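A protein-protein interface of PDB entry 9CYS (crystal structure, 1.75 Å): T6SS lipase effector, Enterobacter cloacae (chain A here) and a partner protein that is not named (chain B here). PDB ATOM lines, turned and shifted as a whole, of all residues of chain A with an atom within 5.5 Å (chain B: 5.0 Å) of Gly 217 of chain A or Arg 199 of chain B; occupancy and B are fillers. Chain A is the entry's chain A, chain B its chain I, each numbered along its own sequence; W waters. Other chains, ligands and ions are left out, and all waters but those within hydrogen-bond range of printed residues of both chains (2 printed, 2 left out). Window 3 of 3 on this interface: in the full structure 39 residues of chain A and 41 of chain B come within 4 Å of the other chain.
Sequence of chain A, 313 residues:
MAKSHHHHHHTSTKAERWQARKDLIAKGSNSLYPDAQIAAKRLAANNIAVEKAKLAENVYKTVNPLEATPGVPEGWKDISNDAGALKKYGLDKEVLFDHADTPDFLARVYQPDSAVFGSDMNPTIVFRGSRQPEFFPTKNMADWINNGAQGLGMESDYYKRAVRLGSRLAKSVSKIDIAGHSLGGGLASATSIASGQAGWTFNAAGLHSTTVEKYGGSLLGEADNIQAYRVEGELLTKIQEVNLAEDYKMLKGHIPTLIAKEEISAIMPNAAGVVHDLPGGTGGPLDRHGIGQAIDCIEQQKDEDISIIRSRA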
ATOM      1  N   ILE A 193      22.619  -1.959 -13.193  1.00  0.00           N
ATOM      2  CA  ILE A 193      22.730  -0.529 -13.471  1.00  0.00           C
ATOM      3  C   ILE A 193      22.061   0.282 -12.367  1.00  0.00           C
ATOM      4  O   ILE A 193      22.599   1.298 -11.905  1.00  0.00           O
ATOM      5  CB  ILE A 193      22.135  -0.193 -14.852  1.00  0.00           C
ATOM      6  CG1 ILE A 193      22.985  -0.796 -15.969  1.00  0.00           C
ATOM      7  CG2 ILE A 193      22.079   1.311 -15.053  1.00  0.00           C
ATOM      8  CD1 ILE A 193      22.240  -0.985 -17.258  1.00  0.00           C
ATOM      9  N   ALA A 194      20.886  -0.167 -11.910  1.00  0.00           N
ATOM     10  CA  ALA A 194      20.148   0.595 -10.902  1.00  0.00           C
ATOM     11  C   ALA A 194      20.849   0.596  -9.552  1.00  0.00           C
ATOM     12  O   ALA A 194      20.751   1.581  -8.810  1.00  0.00           O
ATOM     13  CB  ALA A 194      18.731   0.038 -10.754  1.00  0.00           C
ATOM     14  N   SER A 195      21.543  -0.489  -9.206  1.00  0.00           N
ATOM     15  CA  SER A 195      22.145  -0.625  -7.885  1.00  0.00           C
ATOM     16  C   SER A 195      23.588  -0.167  -7.831  1.00  0.00           C
ATOM     17  O   SER A 195      24.079   0.143  -6.741  1.00  0.00           O
ATOM     18  CB  SER A 195      22.126  -2.076  -7.413  1.00  0.00           C
ATOM     19  OG  SER A 195      22.836  -2.897  -8.338  1.00  0.00           O
ATOM     20  N   GLY A 196      24.290  -0.165  -8.964  1.00  0.00           N
ATOM     21  CA  GLY A 196      25.729   0.009  -8.955  1.00  0.00           C
ATOM     22  C   GLY A 196      26.526  -1.243  -8.666  1.00  0.00           C
ATOM     23  O   GLY A 196      27.765  -1.188  -8.717  1.00  0.00           O
ATOM     24  N   VAL A 212      14.198   1.716 -20.624  1.00  0.00           N
ATOM     25  CA  VAL A 212      15.180   2.675 -20.118  1.00  0.00           C
ATOM     26  C   VAL A 212      14.508   4.007 -19.807  1.00  0.00           C
ATOM     27  O   VAL A 212      14.745   4.613 -18.755  1.00  0.00           O
ATOM     28  CB  VAL A 212      16.334   2.845 -21.122  1.00  0.00           C
ATOM     29  CG1 VAL A 212      17.361   3.830 -20.582  1.00  0.00           C
ATOM     30  CG2 VAL A 212      16.988   1.497 -21.407  1.00  0.00           C
ATOM     31  N   TYR A 215      12.141   3.925 -16.496  1.00  0.00           N
ATOM     32  CA  TYR A 215      12.775   3.949 -15.185  1.00  0.00           C
ATOM     33  C   TYR A 215      13.930   4.941 -15.112  1.00  0.00           C
ATOM     34  O   TYR A 215      14.764   4.849 -14.205  1.00  0.00           O
ATOM     35  CB  TYR A 215      13.226   2.545 -14.790  1.00  0.00           C
ATOM     36  CG  TYR A 215      12.066   1.581 -14.769  1.00  0.00           C
ATOM     37  CD1 TYR A 215      11.278   1.442 -13.633  1.00  0.00           C
ATOM     38  CD2 TYR A 215      11.762   0.808 -15.881  1.00  0.00           C
ATOM     39  CE1 TYR A 215      10.210   0.572 -13.611  1.00  0.00           C
ATOM     40  CE2 TYR A 215      10.704  -0.076 -15.866  1.00  0.00           C
ATOM     41  CZ  TYR A 215       9.929  -0.189 -14.729  1.00  0.00           C
ATOM     42  OH  TYR A 215       8.867  -1.066 -14.715  1.00  0.00           O
ATOM     43  N   GLY A 216      13.991   5.876 -16.057  1.00  0.00           N
ATOM     44  CA  GLY A 216      14.791   7.082 -15.902  1.00  0.00           C
ATOM     45  C   GLY A 216      16.260   6.812 -15.664  1.00  0.00           C
ATOM     46  O   GLY A 216      16.864   5.914 -16.263  1.00  0.00           O
ATOM     47  N   GLY A 217      16.847   7.604 -14.762  1.00  0.00           N
ATOM     48  CA  GLY A 217      18.275   7.540 -14.505  1.00  0.00           C
ATOM     49  C   GLY A 217      18.729   6.256 -13.848  1.00  0.00           C
ATOM     50  O   GLY A 217      19.930   5.952 -13.863  1.00  0.00           O
ATOM     51  N   SER A 218      17.798   5.495 -13.265  1.00  0.00           N
ATOM     52  CA  SER A 218      18.171   4.212 -12.683  1.00  0.00           C
ATOM     53  C   SER A 218      18.708   3.264 -13.741  1.00  0.00           C
ATOM     54  O   SER A 218      19.515   2.382 -13.428  1.00  0.00           O
ATOM     55  CB  SER A 218      16.976   3.584 -11.963  1.00  0.00           C
ATOM     56  OG  SER A 218      16.788   4.177 -10.691  1.00  0.00           O
ATOM     57  N   LEU A 219      18.289   3.438 -14.995  1.00  0.00           N
ATOM     58  CA  LEU A 219      18.742   2.609 -16.104  1.00  0.00           C
ATOM     59  C   LEU A 219      19.666   3.367 -17.053  1.00  0.00           C
ATOM     60  O   LEU A 219      19.875   2.934 -18.191  1.00  0.00           O
ATOM     61  CB  LEU A 219      17.533   2.049 -16.854  1.00  0.00           C
ATOM     62  CG  LEU A 219      16.789   0.950 -16.090  1.00  0.00           C
ATOM     63  CD1 LEU A 219      16.048   0.045 -17.045  1.00  0.00           C
ATOM     64  CD2 LEU A 219      17.757   0.135 -15.231  1.00  0.00           C
ATOM     65  N   LEU A 220      20.235   4.480 -16.598  1.00  0.00           N
ATOM     66  CA  LEU A 220      21.046   5.356 -17.430  1.00  0.00           C
ATOM     67  C   LEU A 220      22.525   5.206 -17.095  1.00  0.00           C
ATOM     68  O   LEU A 220      22.901   5.112 -15.921  1.00  0.00           O
ATOM     69  CB  LEU A 220      20.621   6.816 -17.251  1.00  0.00           C
ATOM     70  CG  LEU A 220      19.393   7.242 -18.057  1.00  0.00           C
ATOM     71  CD1 LEU A 220      19.277   8.751 -18.082  1.00  0.00           C
ATOM     72  CD2 LEU A 220      19.468   6.679 -19.467  1.00  0.00           C
ATOM     73  N   ARG B 195      19.590  10.536  -4.217  1.00  0.00           N
ATOM     74  CA  ARG B 195      20.352   9.690  -5.126  1.00  0.00           C
ATOM     75  C   ARG B 195      19.712   9.636  -6.508  1.00  0.00           C
ATOM     76  O   ARG B 195      20.407   9.753  -7.526  1.00  0.00           O
ATOM     77  CB  ARG B 195      20.496   8.292  -4.517  1.00  0.00           C
ATOM     78  CG  ARG B 195      21.314   7.318  -5.336  1.00  0.00           C
ATOM     79  CD  ARG B 195      21.583   6.021  -4.586  1.00  0.00           C
ATOM     80  NE  ARG B 195      22.100   5.016  -5.504  1.00  0.00           N
ATOM     81  CZ  ARG B 195      21.351   4.337  -6.358  1.00  0.00           C
ATOM     82  NH1 ARG B 195      20.027   4.438  -6.350  1.00  0.00           N
ATOM     83  NH2 ARG B 195      21.942   3.544  -7.249  1.00  0.00           N
ATOM     84  N   PHE B 196      18.386   9.475  -6.571  1.00  0.00           N
ATOM     85  CA  PHE B 196      17.699   9.455  -7.860  1.00  0.00           C
ATOM     86  C   PHE B 196      17.884  10.781  -8.593  1.00  0.00           C
ATOM     87  O   PHE B 196      18.159  10.809  -9.798  1.00  0.00           O
ATOM     88  CB  PHE B 196      16.206   9.174  -7.665  1.00  0.00           C
ATOM     89  CG  PHE B 196      15.872   7.725  -7.423  1.00  0.00           C
ATOM     90  CD1 PHE B 196      16.869   6.770  -7.270  1.00  0.00           C
ATOM     91  CD2 PHE B 196      14.544   7.322  -7.342  1.00  0.00           C
ATOM     92  CE1 PHE B 196      16.547   5.437  -7.046  1.00  0.00           C
ATOM     93  CE2 PHE B 196      14.214   5.989  -7.118  1.00  0.00           C
ATOM     94  CZ  PHE B 196      15.218   5.046  -6.974  1.00  0.00           C
ATOM     95  N   LEU B 197      17.717  11.893  -7.877  1.00  0.00           N
ATOM     96  CA  LEU B 197      17.878  13.209  -8.488  1.00  0.00           C
ATOM     97  C   LEU B 197      19.298  13.404  -9.017  1.00  0.00           C
ATOM     98  O   LEU B 197      19.488  13.974 -10.096  1.00  0.00           O
ATOM     99  CB  LEU B 197      17.519  14.297  -7.477  1.00  0.00           C
ATOM    100  CG  LEU B 197      16.030  14.610  -7.291  1.00  0.00           C
ATOM    101  CD1 LEU B 197      15.775  15.230  -5.922  1.00  0.00           C
ATOM    102  CD2 LEU B 197      15.536  15.526  -8.390  1.00  0.00           C
ATOM    103  N   ASP B 198      20.304  12.922  -8.277  1.00  0.00           N
ATOM    104  CA  ASP B 198      21.688  13.022  -8.743  1.00  0.00           C
ATOM    105  C   ASP B 198      21.942  12.197 -10.002  1.00  0.00           C
ATOM    106  O   ASP B 198      22.849  12.521 -10.777  1.00  0.00           O
ATOM    107  CB  ASP B 198      22.657  12.578  -7.650  1.00  0.00           C
ATOM    108  CG  ASP B 198      22.780  13.581  -6.528  1.00  0.00           C
ATOM    109  OD1 ASP B 198      22.310  14.723  -6.691  1.00  0.00           O
ATOM    110  OD2 ASP B 198      23.356  13.221  -5.475  1.00  0.00           O
ATOM    111  N   ARG B 199      21.174  11.132 -10.226  1.00  0.00           N
ATOM    112  CA  ARG B 199      21.372  10.280 -11.391  1.00  0.00           C
ATOM    113  C   ARG B 199      20.441  10.612 -12.547  1.00  0.00           C
ATOM    114  O   ARG B 199      20.653  10.110 -13.655  1.00  0.00           O
ATOM    115  CB  ARG B 199      21.196   8.807 -11.005  1.00  0.00           C
ATOM    116  CG  ARG B 199      22.234   8.321 -10.009  1.00  0.00           C
ATOM    117  CD  ARG B 199      21.886   6.954  -9.455  1.00  0.00           C
ATOM    118  NE  ARG B 199      21.552   6.005 -10.515  1.00  0.00           N
ATOM    119  CZ  ARG B 199      22.321   4.992 -10.891  1.00  0.00           C
ATOM    120  NH1 ARG B 199      23.515   4.796 -10.356  1.00  0.00           N
ATOM    121  NH2 ARG B 199      21.886   4.160 -11.833  1.00  0.00           N
ATOM    122  N   ALA B 200      19.425  11.437 -12.328  1.00  0.00           N
ATOM    123  CA  ALA B 200      18.467  11.714 -13.386  1.00  0.00           C
ATOM    124  C   ALA B 200      19.052  12.688 -14.405  1.00  0.00           C
ATOM    125  O   ALA B 200      20.003  13.427 -14.132  1.00  0.00           O
ATOM    126  CB  ALA B 200      17.168  12.278 -12.810  1.00  0.00           C
ATOM    127  N   LYS B 201      18.467  12.671 -15.599  1.00  0.00           N
ATOM    128  CA  LYS B 201      18.841  13.578 -16.676  1.00  0.00           C
ATOM    129  C   LYS B 201      18.070  14.882 -16.504  1.00  0.00           C
ATOM    130  O   LYS B 201      16.834  14.875 -16.486  1.00  0.00           O
ATOM    131  CB  LYS B 201      18.543  12.933 -18.030  1.00  0.00           C
ATOM    132  CG  LYS B 201      18.956  13.746 -19.246  1.00  0.00           C
ATOM    133  CD  LYS B 201      18.320  13.171 -20.508  1.00  0.00           C
ATOM    134  CE  LYS B 201      18.751  13.931 -21.755  1.00  0.00           C
ATOM    135  NZ  LYS B 201      19.645  15.080 -21.431  1.00  0.00           N
ATOM    136  N   GLU B 206      11.384  12.263 -16.021  1.00  0.00           N
ATOM    137  CA  GLU B 206      11.639  11.655 -14.724  1.00  0.00           C
ATOM    138  C   GLU B 206      12.231  12.672 -13.757  1.00  0.00           C
ATOM    139  O   GLU B 206      11.910  12.666 -12.564  1.00  0.00           O
ATOM    140  CB  GLU B 206      12.568  10.455 -14.892  1.00  0.00           C
ATOM    141  CG  GLU B 206      12.432   9.417 -13.799  1.00  0.00           C
ATOM    142  CD  GLU B 206      13.759   9.073 -13.168  1.00  0.00           C
ATOM    143  OE1 GLU B 206      14.806   9.541 -13.674  1.00  0.00           O
ATOM    144  OE2 GLU B 206      13.756   8.330 -12.164  1.00  0.00           O
HETATM  145  O   HOH W   1      18.646   3.352  -8.575  1.00  0.00           O
HETATM  146  O   HOH W   2      18.453   6.516 -10.359  1.00  0.00           O
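The guanidinium group of Arg 199 of chain B sits at hydrogen-bond distance from the backbone carbonyl oxygen of Ile 193 of chain A (3.0 Å). The side-chain carboxylate of Glu 206 of chain B lies within hydrogen-bond range of the backbone NH of Gly 217 of chain A, at 3.0 Å. NH2 of Arg 199 of chain B is in hydrogen-bond range of O of Gly 217 of chain A, 3.3 Å away. The guanidinium group of Arg 199 of chain B is in hydrogen-bond range of the backbone carbonyl oxygen of Ser 218 of chain A (3.4 Å). O of Ala 194 of chain A lies within hydrogen-bond range of NH2 of Arg 195 of chain B (2.8 Å).
N of Ala 194 of chain A sits close to O of Ser 218 of chain A (3.3 Å).
Among the printed residues, merely in contact across the chains: Gly 216 of chain A with Glu 206 of chain B and Ser 218 of chain A with Phe 196 of chain B.
Of chain B, only Arg 199 (3.3 Å) and Glu 206 (3.0 Å) come within 4 Å of Gly 217 of chain A. Of chain A, only Ile 193 (3.0 Å), Gly 217 (3.3 Å) and Ser 218 (3.4 Å) come within 4 Å of Arg 199 of chain B. Of the printed residues of chain B, Ile 193 of chain A touches Arg 199. Of the printed residues of chain B, Gly 216 of chain A touches Glu 206 (3.3 Å). The nearest residue of chain A that does not touch Arg 199 of chain B is Ala 194 of chain A (4.1 Å).
Of the 11 printed residues of chain A, 5 touch a printed residue of chain B. Printed residues of chain A that touch a printed residue of chain B: Ile 193, Ala 194, Gly 216, Gly 217 and Ser 218. Along chain A the printed residues that touch a printed residue of chain B span positions 193 to 218. Among the printed residues, 7 pairs touch across the chains. Among the printed residues, no Asp or Glu carboxylate lies within 4 Å of a Lys or Arg side-chain nitrogen of the other chain.
Water W1 lies within hydrogen-bond range of the backbone carbonyl oxygen of Ala 194 of chain A (2.8 Å), the guanidinium group of Arg 195 of chain B (2.8 Å) and the side-chain hydroxyl of Ser 218 of chain A (2.9 Å). Water W2 bridges the side-chain hydroxyl (OG) of Ser 218 of chain A and the guanidinium group (NE) of Arg 199 of chain B.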
